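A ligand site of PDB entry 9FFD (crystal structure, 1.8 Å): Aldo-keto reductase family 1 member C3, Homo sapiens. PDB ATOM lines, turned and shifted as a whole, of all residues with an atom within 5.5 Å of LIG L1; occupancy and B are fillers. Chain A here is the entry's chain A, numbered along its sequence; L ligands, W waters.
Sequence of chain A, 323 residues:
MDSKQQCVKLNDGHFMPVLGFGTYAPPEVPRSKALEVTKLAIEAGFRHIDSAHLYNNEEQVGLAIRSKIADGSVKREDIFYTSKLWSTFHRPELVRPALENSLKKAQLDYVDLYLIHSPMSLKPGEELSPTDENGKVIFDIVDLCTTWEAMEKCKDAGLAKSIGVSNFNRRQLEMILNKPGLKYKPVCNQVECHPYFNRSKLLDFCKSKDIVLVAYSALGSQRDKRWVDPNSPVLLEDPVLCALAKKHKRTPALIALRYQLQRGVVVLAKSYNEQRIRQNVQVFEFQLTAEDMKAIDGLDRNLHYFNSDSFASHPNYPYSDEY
O14 of LG2 L2 is in hydrogen-bond range of ND2 of Asn 167 (2.9 Å).
The side-chain hydroxyl (OH) of Tyr 55 sits at hydrogen-bond distance from an oxygen (O2) of LIG L1 (2.5 Å).
An oxygen (O2) of LIG L1 is in hydrogen-bond range of a ring nitrogen (NE2) of His 117, 2.7 Å away.
The backbone NH of Tyr 24 sits at hydrogen-bond distance from an oxygen (O12) of LG2 L2 (3.1 Å).
Water W1 lies within hydrogen-bond range of OH of Tyr 24 (2.7 Å), OD1 of Asp 224 (2.7 Å), NE1 of Trp 227 (3.2 Å) and O3 of LIG L1 (3.4 Å).
CE2 of Tyr 24 touches O3 of LIG L1, at 3.1 Å.
CD2 of Leu 54 touches C3 of LIG L1, at 3.4 Å.
CE of Met 120 touches C9 of LIG L1, 3.9 Å away.
OD1 of Asn 167 touches C18 of LIG L1, at 3.6 Å.
OH of Tyr 216 touches C18 of LIG L1, 3.5 Å away.
Trp 227 touches LIG L1.
Phe 306 touches LIG L1.
Phe 311 touches LIG L1.
Pro 318 touches LIG L1 (CG to BR1, 3.3 Å).
Tyr 319 touches LIG L1.
Hydrophobic or aromatic side chains within 4 Å of LIG L1: Tyr 24, Leu 54, Tyr 55, His 117, Met 120, Trp 227, Phe 306, Phe 311, Pro 318 and Tyr 319.
Of the 18 residues printed, 12 come within 4 Å of LIG L1.
An oxygen (O2) of LIG L1 lies close to an oxygen (O14) of LG2 L2.
O of His 117 is in hydrogen-bond range of ND2 of Asn 167, 2.9 Å away.
The side-chain hydroxyl of Tyr 216 is in hydrogen-bond range of the side-chain amide oxygen of Asn 167, 2.6 Å away.
The side-chain hydroxyl (OH) of Tyr 55 is in hydrogen-bond range of the side-chain amino group (NZ) of Lys 84 (3.0 Å).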
ATOM      1  N   TYR A  24      -2.930   6.402  31.261  1.00  0.00           N
ATOM      2  CA  TYR A  24      -1.807   6.769  30.406  1.00  0.00           C
ATOM      3  C   TYR A  24      -0.885   7.740  31.119  1.00  0.00           C
ATOM      4  O   TYR A  24      -1.349   8.689  31.761  1.00  0.00           O
ATOM      5  CB  TYR A  24      -2.276   7.381  29.096  1.00  0.00           C
ATOM      6  CG  TYR A  24      -1.066   7.779  28.272  1.00  0.00           C
ATOM      7  CD1 TYR A  24      -0.346   6.828  27.566  1.00  0.00           C
ATOM      8  CD2 TYR A  24      -0.617   9.103  28.244  1.00  0.00           C
ATOM      9  CE1 TYR A  24       0.765   7.173  26.837  1.00  0.00           C
ATOM     10  CE2 TYR A  24       0.508   9.445  27.513  1.00  0.00           C
ATOM     11  CZ  TYR A  24       1.194   8.472  26.814  1.00  0.00           C
ATOM     12  OH  TYR A  24       2.302   8.785  26.067  1.00  0.00           O
ATOM     13  N   LEU A  54      -1.275   0.589  23.375  1.00  0.00           N
ATOM     14  CA  LEU A  54      -0.391   1.708  23.073  1.00  0.00           C
ATOM     15  C   LEU A  54       0.302   2.260  24.305  1.00  0.00           C
ATOM     16  O   LEU A  54       1.414   2.807  24.207  1.00  0.00           O
ATOM     17  CB  LEU A  54      -1.185   2.821  22.392  1.00  0.00           C
ATOM     18  CG  LEU A  54      -0.423   4.057  21.929  1.00  0.00           C
ATOM     19  CD1 LEU A  54       0.440   3.722  20.723  1.00  0.00           C
ATOM     20  CD2 LEU A  54      -1.381   5.189  21.610  1.00  0.00           C
ATOM     21  N   TYR A  55      -0.319   2.138  25.475  1.00  0.00           N
ATOM     22  CA  TYR A  55       0.161   2.853  26.660  1.00  0.00           C
ATOM     23  C   TYR A  55       1.356   2.204  27.326  1.00  0.00           C
ATOM     24  O   TYR A  55       1.896   2.790  28.273  1.00  0.00           O
ATOM     25  CB  TYR A  55      -0.968   2.965  27.699  1.00  0.00           C
ATOM     26  CG  TYR A  55      -2.217   3.673  27.234  1.00  0.00           C
ATOM     27  CD1 TYR A  55      -2.232   4.405  26.060  1.00  0.00           C
ATOM     28  CD2 TYR A  55      -3.375   3.616  27.986  1.00  0.00           C
ATOM     29  CE1 TYR A  55      -3.379   5.060  25.641  1.00  0.00           C
ATOM     30  CE2 TYR A  55      -4.523   4.263  27.581  1.00  0.00           C
ATOM     31  CZ  TYR A  55      -4.516   4.987  26.417  1.00  0.00           C
ATOM     32  OH  TYR A  55      -5.668   5.610  26.026  1.00  0.00           O
ATOM     33  N   LYS A  84      -7.484  -1.619  24.336  1.00  0.00           N
ATOM     34  CA  LYS A  84      -7.741  -1.064  23.013  1.00  0.00           C
ATOM     35  C   LYS A  84      -6.819  -1.682  21.983  1.00  0.00           C
ATOM     36  O   LYS A  84      -5.626  -1.883  22.220  1.00  0.00           O
ATOM     37  CB  LYS A  84      -7.585   0.457  22.988  1.00  0.00           C
ATOM     38  CG  LYS A  84      -8.317   1.197  24.104  1.00  0.00           C
ATOM     39  CD  LYS A  84      -8.339   2.678  23.859  1.00  0.00           C
ATOM     40  CE  LYS A  84      -8.865   3.426  25.067  1.00  0.00           C
ATOM     41  NZ  LYS A  84      -7.814   3.549  26.129  1.00  0.00           N
ATOM     42  N   TRP A  86      -4.670  -1.476  18.866  1.00  0.00           N
ATOM     43  CA  TRP A  86      -3.918  -0.396  18.241  1.00  0.00           C
ATOM     44  C   TRP A  86      -4.028  -0.526  16.718  1.00  0.00           C
ATOM     45  O   TRP A  86      -4.388  -1.571  16.170  1.00  0.00           O
ATOM     46  CB  TRP A  86      -2.455  -0.385  18.718  1.00  0.00           C
ATOM     47  CG  TRP A  86      -1.746   0.779  18.099  1.00  0.00           C
ATOM     48  CD1 TRP A  86      -0.655   0.723  17.293  1.00  0.00           C
ATOM     49  CD2 TRP A  86      -2.126   2.162  18.150  1.00  0.00           C
ATOM     50  NE1 TRP A  86      -0.320   1.981  16.848  1.00  0.00           N
ATOM     51  CE2 TRP A  86      -1.213   2.876  17.352  1.00  0.00           C
ATOM     52  CE3 TRP A  86      -3.166   2.857  18.786  1.00  0.00           C
ATOM     53  CZ2 TRP A  86      -1.296   4.254  17.194  1.00  0.00           C
ATOM     54  CZ3 TRP A  86      -3.246   4.230  18.607  1.00  0.00           C
ATOM     55  CH2 TRP A  86      -2.318   4.908  17.823  1.00  0.00           C
ATOM     56  N   HIS A 117      -9.037   1.443  18.841  1.00  0.00           N
ATOM     57  CA  HIS A 117      -8.471   2.658  19.437  1.00  0.00           C
ATOM     58  C   HIS A 117      -8.687   3.877  18.560  1.00  0.00           C
ATOM     59  O   HIS A 117      -8.911   4.990  19.064  1.00  0.00           O
ATOM     60  CB  HIS A 117      -6.976   2.440  19.709  1.00  0.00           C
ATOM     61  CG  HIS A 117      -6.397   3.347  20.755  1.00  0.00           C
ATOM     62  ND1 HIS A 117      -5.342   2.967  21.556  1.00  0.00           N
ATOM     63  CD2 HIS A 117      -6.708   4.611  21.130  1.00  0.00           C
ATOM     64  CE1 HIS A 117      -5.040   3.940  22.379  1.00  0.00           C
ATOM     65  NE2 HIS A 117      -5.854   4.960  22.145  1.00  0.00           N
ATOM     66  N   MET A 120      -7.921   5.315  12.252  1.00  0.00           N
ATOM     67  CA  MET A 120      -6.814   5.644  11.350  1.00  0.00           C
ATOM     68  C   MET A 120      -5.836   4.471  11.275  1.00  0.00           C
ATOM     69  O   MET A 120      -4.781   4.446  11.917  1.00  0.00           O
ATOM     70  CB  MET A 120      -6.128   6.921  11.830  1.00  0.00           C
ATOM     71  CG  MET A 120      -7.006   8.159  11.678  1.00  0.00           C
ATOM     72  SD  MET A 120      -6.142   9.683  12.063  1.00  0.00           S
ATOM     73  CE  MET A 120      -5.874   9.517  13.824  1.00  0.00           C
ATOM     74  N   ASN A 167     -12.674   7.338  18.954  1.00  0.00           N
ATOM     75  CA  ASN A 167     -12.257   8.348  17.993  1.00  0.00           C
ATOM     76  C   ASN A 167     -12.998   8.240  16.675  1.00  0.00           C
ATOM     77  O   ASN A 167     -12.496   8.709  15.643  1.00  0.00           O
ATOM     78  CB  ASN A 167     -10.751   8.285  17.790  1.00  0.00           C
ATOM     79  CG  ASN A 167      -9.977   8.729  19.019  1.00  0.00           C
ATOM     80  OD1 ASN A 167     -10.198   9.821  19.532  1.00  0.00           O
ATOM     81  ND2 ASN A 167      -9.087   7.869  19.521  1.00  0.00           N
ATOM     82  N   TYR A 216     -12.639  11.290  27.083  1.00  0.00           N
ATOM     83  CA  TYR A 216     -11.246  11.380  27.483  1.00  0.00           C
ATOM     84  C   TYR A 216     -10.741  12.815  27.365  1.00  0.00           C
ATOM     85  O   TYR A 216     -11.353  13.661  26.708  1.00  0.00           O
ATOM     86  CB  TYR A 216     -10.351  10.418  26.670  1.00  0.00           C
ATOM     87  CG  TYR A 216     -10.043  10.716  25.223  1.00  0.00           C
ATOM     88  CD1 TYR A 216      -9.159  11.744  24.874  1.00  0.00           C
ATOM     89  CD2 TYR A 216     -10.527   9.907  24.197  1.00  0.00           C
ATOM     90  CE1 TYR A 216      -8.841  11.990  23.564  1.00  0.00           C
ATOM     91  CE2 TYR A 216     -10.211  10.140  22.893  1.00  0.00           C
ATOM     92  CZ  TYR A 216      -9.363  11.187  22.567  1.00  0.00           C
ATOM     93  OH  TYR A 216      -9.029  11.433  21.263  1.00  0.00           O
ATOM     94  N   ASP A 224       0.954  17.185  26.806  1.00  0.00           N
ATOM     95  CA  ASP A 224       2.249  16.733  26.341  1.00  0.00           C
ATOM     96  C   ASP A 224       2.715  17.585  25.159  1.00  0.00           C
ATOM     97  O   ASP A 224       2.031  17.639  24.125  1.00  0.00           O
ATOM     98  CB  ASP A 224       2.162  15.259  25.941  1.00  0.00           C
ATOM     99  CG  ASP A 224       3.515  14.630  25.716  1.00  0.00           C
ATOM    100  OD1 ASP A 224       3.824  13.630  26.398  1.00  0.00           O
ATOM    101  OD2 ASP A 224       4.277  15.126  24.879  1.00  0.00           O
ATOM    102  N   TRP A 227       2.393  16.587  21.445  1.00  0.00           N
ATOM    103  CA  TRP A 227       1.120  16.387  20.771  1.00  0.00           C
ATOM    104  C   TRP A 227       0.100  17.490  21.004  1.00  0.00           C
ATOM    105  O   TRP A 227      -0.921  17.508  20.299  1.00  0.00           O
ATOM    106  CB  TRP A 227       0.485  15.058  21.212  1.00  0.00           C
ATOM    107  CG  TRP A 227       1.476  13.955  21.384  1.00  0.00           C
ATOM    108  CD1 TRP A 227       1.934  13.448  22.566  1.00  0.00           C
ATOM    109  CD2 TRP A 227       2.139  13.229  20.347  1.00  0.00           C
ATOM    110  NE1 TRP A 227       2.838  12.439  22.330  1.00  0.00           N
ATOM    111  CE2 TRP A 227       2.988  12.290  20.977  1.00  0.00           C
ATOM    112  CE3 TRP A 227       2.109  13.282  18.955  1.00  0.00           C
ATOM    113  CZ2 TRP A 227       3.784  11.411  20.251  1.00  0.00           C
ATOM    114  CZ3 TRP A 227       2.902  12.415  18.236  1.00  0.00           C
ATOM    115  CH2 TRP A 227       3.733  11.483  18.889  1.00  0.00           C
ATOM    116  N   PHE A 306      -5.494  17.214  21.106  1.00  0.00           N
ATOM    117  CA  PHE A 306      -4.685  16.433  20.172  1.00  0.00           C
ATOM    118  C   PHE A 306      -4.961  16.933  18.753  1.00  0.00           C
ATOM    119  O   PHE A 306      -6.038  16.692  18.198  1.00  0.00           O
ATOM    120  CB  PHE A 306      -4.999  14.951  20.320  1.00  0.00           C
ATOM    121  CG  PHE A 306      -4.636  14.424  21.661  1.00  0.00           C
ATOM    122  CD1 PHE A 306      -3.359  13.957  21.901  1.00  0.00           C
ATOM    123  CD2 PHE A 306      -5.559  14.425  22.688  1.00  0.00           C
ATOM    124  CE1 PHE A 306      -3.014  13.491  23.149  1.00  0.00           C
ATOM    125  CE2 PHE A 306      -5.223  13.955  23.941  1.00  0.00           C
ATOM    126  CZ  PHE A 306      -3.951  13.496  24.178  1.00  0.00           C
ATOM    127  N   ASN A 307      -3.963  17.618  18.164  1.00  0.00           N
ATOM    128  CA  ASN A 307      -4.156  18.245  16.846  1.00  0.00           C
ATOM    129  C   ASN A 307      -2.783  18.352  16.176  1.00  0.00           C
ATOM    130  O   ASN A 307      -2.157  19.412  16.115  1.00  0.00           O
ATOM    131  CB  ASN A 307      -4.816  19.618  16.973  1.00  0.00           C
ATOM    132  CG  ASN A 307      -5.474  20.065  15.677  1.00  0.00           C
ATOM    133  OD1 ASN A 307      -6.597  19.675  15.363  1.00  0.00           O
ATOM    134  ND2 ASN A 307      -4.776  20.918  14.925  1.00  0.00           N
ATOM    135  N   SER A 308      -2.309  17.220  15.652  1.00  0.00           N
ATOM    136  CA  SER A 308      -1.113  17.180  14.824  1.00  0.00           C
ATOM    137  C   SER A 308      -1.498  17.064  13.363  1.00  0.00           C
ATOM    138  O   SER A 308      -2.422  16.335  13.001  1.00  0.00           O
ATOM    139  CB  SER A 308      -0.200  16.014  15.216  1.00  0.00           C
ATOM    140  OG  SER A 308       0.561  16.327  16.375  1.00  0.00           O
ATOM    141  N   PHE A 311      -1.609  13.545  11.226  1.00  0.00           N
ATOM    142  CA  PHE A 311      -2.776  12.685  11.079  1.00  0.00           C
ATOM    143  C   PHE A 311      -3.910  13.323  10.278  1.00  0.00           C
ATOM    144  O   PHE A 311      -4.794  12.603   9.810  1.00  0.00           O
ATOM    145  CB  PHE A 311      -3.329  12.280  12.445  1.00  0.00           C
ATOM    146  CG  PHE A 311      -2.277  12.101  13.503  1.00  0.00           C
ATOM    147  CD1 PHE A 311      -2.240  12.934  14.608  1.00  0.00           C
ATOM    148  CD2 PHE A 311      -1.321  11.115  13.390  1.00  0.00           C
ATOM    149  CE1 PHE A 311      -1.267  12.777  15.584  1.00  0.00           C
ATOM    150  CE2 PHE A 311      -0.342  10.957  14.353  1.00  0.00           C
ATOM    151  CZ  PHE A 311      -0.313  11.794  15.447  1.00  0.00           C
ATOM    152  N   TYR A 317      -9.129  10.251   9.060  1.00  0.00           N
ATOM    153  CA  TYR A 317      -9.110  11.275  10.090  1.00  0.00           C
ATOM    154  C   TYR A 317     -10.542  11.677  10.454  1.00  0.00           C
ATOM    155  O   TYR A 317     -11.328  12.029   9.565  1.00  0.00           O
ATOM    156  CB  TYR A 317      -8.313  12.480   9.565  1.00  0.00           C
ATOM    157  CG  TYR A 317      -8.056  13.595  10.549  1.00  0.00           C
ATOM    158  CD1 TYR A 317      -7.184  13.422  11.626  1.00  0.00           C
ATOM    159  CD2 TYR A 317      -8.645  14.844  10.387  1.00  0.00           C
ATOM    160  CE1 TYR A 317      -6.939  14.450  12.517  1.00  0.00           C
ATOM    161  CE2 TYR A 317      -8.408  15.876  11.267  1.00  0.00           C
ATOM    162  CZ  TYR A 317      -7.553  15.673  12.329  1.00  0.00           C
ATOM    163  OH  TYR A 317      -7.322  16.714  13.207  1.00  0.00           O
ATOM    164  N   PRO A 318     -10.922  11.605  11.732  1.00  0.00           N
ATOM    165  CA  PRO A 318     -12.347  11.765  12.072  1.00  0.00           C
ATOM    166  C   PRO A 318     -12.826  13.210  12.142  1.00  0.00           C
ATOM    167  O   PRO A 318     -14.052  13.422  12.146  1.00  0.00           O
ATOM    168  CB  PRO A 318     -12.444  11.095  13.461  1.00  0.00           C
ATOM    169  CG  PRO A 318     -11.076  11.327  14.061  1.00  0.00           C
ATOM    170  CD  PRO A 318     -10.107  11.205  12.897  1.00  0.00           C
ATOM    171  N   TYR A 319     -11.933  14.199  12.184  1.00  0.00           N
ATOM    172  CA  TYR A 319     -12.336  15.586  12.387  1.00  0.00           C
ATOM    173  C   TYR A 319     -12.506  16.357  11.074  1.00  0.00           C
ATOM    174  O   TYR A 319     -12.633  17.586  11.112  1.00  0.00           O
ATOM    175  CB  TYR A 319     -11.331  16.308  13.288  1.00  0.00           C
ATOM    176  CG  TYR A 319     -11.222  15.764  14.701  1.00  0.00           C
ATOM    177  CD1 TYR A 319     -12.303  15.141  15.316  1.00  0.00           C
ATOM    178  CD2 TYR A 319     -10.035  15.867  15.420  1.00  0.00           C
ATOM    179  CE1 TYR A 319     -12.205  14.642  16.608  1.00  0.00           C
ATOM    180  CE2 TYR A 319      -9.929  15.372  16.708  1.00  0.00           C
ATOM    181  CZ  TYR A 319     -11.018  14.761  17.297  1.00  0.00           C
ATOM    182  OH  TYR A 319     -10.914  14.262  18.576  1.00  0.00           O
HETATM  183  N1  LIG L   1      -0.978  10.449  19.686  1.00  0.00           N
HETATM  184  C1  LIG L   1      -3.468   8.489  24.417  1.00  0.00           C
HETATM  185  C2  LIG L   1      -4.126   7.658  23.514  1.00  0.00           C
HETATM  186  C3  LIG L   1      -3.688   7.581  22.190  1.00  0.00           C
HETATM  187  C4  LIG L   1      -0.787  10.021  22.261  1.00  0.00           C
HETATM  188  C5  LIG L   1      -0.180  10.802  23.156  1.00  0.00           C
HETATM  189  C6  LIG L   1      -3.937   8.557  25.866  1.00  0.00           C
HETATM  190  C7  LIG L   1      -1.124  11.906  19.858  1.00  0.00           C
HETATM  191  C8  LIG L   1      -4.609  11.508  18.486  1.00  0.00           C
HETATM  192  C9  LIG L   1      -5.961  12.271  16.636  1.00  0.00           C
HETATM  193  C10 LIG L   1      -5.733  10.900  19.082  1.00  0.00           C
HETATM  194  C11 LIG L   1      -5.682  10.150  20.404  1.00  0.00           C
HETATM  195  C12 LIG L   1      -2.608   8.335  21.763  1.00  0.00           C
HETATM  196  C13 LIG L   1      -0.292   9.876  20.830  1.00  0.00           C
HETATM  197  C14 LIG L   1      -0.342  10.036  18.416  1.00  0.00           C
HETATM  198  C15 LIG L   1      -2.379  12.365  19.117  1.00  0.00           C
HETATM  199  C16 LIG L   1      -4.718  12.183  17.261  1.00  0.00           C
HETATM  200  C17 LIG L   1      -7.059  11.672  17.244  1.00  0.00           C
HETATM  201  C18 LIG L   1      -6.951  11.001  18.445  1.00  0.00           C
HETATM  202  C19 LIG L   1      -1.933   9.175  22.658  1.00  0.00           C
HETATM  203  C20 LIG L   1      -2.371   9.252  23.982  1.00  0.00           C
HETATM  204  C21 LIG L   1      -0.635  10.870  24.534  1.00  0.00           C
HETATM  205  N2  LIG L   1      -3.344  11.438  19.075  1.00  0.00           N
HETATM  206  O1  LIG L   1      -1.718  10.083  24.898  1.00  0.00           O
HETATM  207  O2  LIG L   1      -5.191   6.884  23.879  1.00  0.00           O
HETATM  208  O3  LIG L   1      -0.140  11.569  25.416  1.00  0.00           O
HETATM  209  O4  LIG L   1      -2.445  13.493  18.631  1.00  0.00           O
HETATM  210 BR1  LIG L   1      -8.779  11.729  16.459  1.00  0.00          BR
HETATM  211  P1  LG2 L   2      -7.098  14.016  31.803  1.00  0.00           P
HETATM  212  O1  LG2 L   2      -8.027  13.031  32.450  1.00  0.00           O
HETATM  213  O2  LG2 L   2      -7.663  15.055  30.929  1.00  0.00           O
HETATM  214  O3  LG2 L   2      -6.192  14.697  32.931  1.00  0.00           O
HETATM  215  C1  LG2 L   2      -5.291  15.772  32.567  1.00  0.00           C
HETATM  216  C2  LG2 L   2      -4.470  16.120  33.784  1.00  0.00           C
HETATM  217  O4  LG2 L   2      -5.356  16.515  34.865  1.00  0.00           O
HETATM  218  C3  LG2 L   2      -3.689  14.945  34.373  1.00  0.00           C
HETATM  219  O5  LG2 L   2      -2.348  14.863  33.903  1.00  0.00           O
HETATM  220  C4  LG2 L   2      -3.758  15.126  35.895  1.00  0.00           C
HETATM  221  O6  LG2 L   2      -2.474  15.457  36.435  1.00  0.00           O
HETATM  222  C5  LG2 L   2      -4.660  16.335  36.081  1.00  0.00           C
HETATM  223  N1  LG2 L   2      -5.650  16.183  37.131  1.00  0.00           N
HETATM  224  C6  LG2 L   2      -6.333  15.035  37.452  1.00  0.00           C
HETATM  225  N2  LG2 L   2      -7.169  15.186  38.443  1.00  0.00           N
HETATM  226  C7  LG2 L   2      -7.043  16.515  38.813  1.00  0.00           C
HETATM  227  C8  LG2 L   2      -7.662  17.287  39.817  1.00  0.00           C
HETATM  228  N3  LG2 L   2      -8.575  16.810  40.649  1.00  0.00           N
HETATM  229  N4  LG2 L   2      -7.291  18.584  39.924  1.00  0.00           N
HETATM  230  C9  LG2 L   2      -6.376  19.057  39.070  1.00  0.00           C
HETATM  231  N5  LG2 L   2      -5.723  18.429  38.090  1.00  0.00           N
HETATM  232  C10 LG2 L   2      -6.095  17.141  38.014  1.00  0.00           C
HETATM  233  O7  LG2 L   2      -5.955  13.231  31.002  1.00  0.00           O
HETATM  234  P2  LG2 L   2      -5.826  12.313  29.691  1.00  0.00           P
HETATM  235  O8  LG2 L   2      -4.749  11.328  30.012  1.00  0.00           O
HETATM  236  O9  LG2 L   2      -5.655  13.170  28.501  1.00  0.00           O
HETATM  237  O10 LG2 L   2      -7.248  11.586  29.578  1.00  0.00           O
HETATM  238  C11 LG2 L   2      -7.546  10.621  30.578  1.00  0.00           C
HETATM  239  C12 LG2 L   2      -7.382   9.217  30.036  1.00  0.00           C
HETATM  240  O11 LG2 L   2      -8.325   9.012  28.952  1.00  0.00           O
HETATM  241  C13 LG2 L   2      -6.053   8.660  29.476  1.00  0.00           C
HETATM  242  O12 LG2 L   2      -5.207   8.420  30.603  1.00  0.00           O
HETATM  243  C14 LG2 L   2      -6.605   7.440  28.708  1.00  0.00           C
HETATM  244  O13 LG2 L   2      -6.848   6.425  29.662  1.00  0.00           O
HETATM  245  C15 LG2 L   2      -7.852   8.030  28.050  1.00  0.00           C
HETATM  246  N6  LG2 L   2      -7.493   8.583  26.707  1.00  0.00           N
HETATM  247  C16 LG2 L   2      -7.870   7.900  25.560  1.00  0.00           C
HETATM  248  C17 LG2 L   2      -7.536   8.400  24.306  1.00  0.00           C
HETATM  249  C18 LG2 L   2      -8.014   7.676  23.090  1.00  0.00           C
HETATM  250  O14 LG2 L   2      -7.602   8.020  21.971  1.00  0.00           O
HETATM  251  N7  LG2 L   2      -8.952   6.756  23.254  1.00  0.00           N
HETATM  252  C19 LG2 L   2      -6.825   9.582  24.200  1.00  0.00           C
HETATM  253  C20 LG2 L   2      -6.449  10.252  25.354  1.00  0.00           C
HETATM  254  C21 LG2 L   2      -6.780   9.749  26.586  1.00  0.00           C
HETATM  255  P3  LG2 L   2      -1.899  14.603  37.696  1.00  0.00           P
HETATM  256  O15 LG2 L   2      -2.977  14.558  38.762  1.00  0.00           O
HETATM  257  O16 LG2 L   2      -1.529  13.239  37.184  1.00  0.00           O
HETATM  258  O17 LG2 L   2      -0.673  15.397  38.155  1.00  0.00           O
HETATM  259  O   HOH W   1       3.267  11.196  25.278  1.00  0.00           O
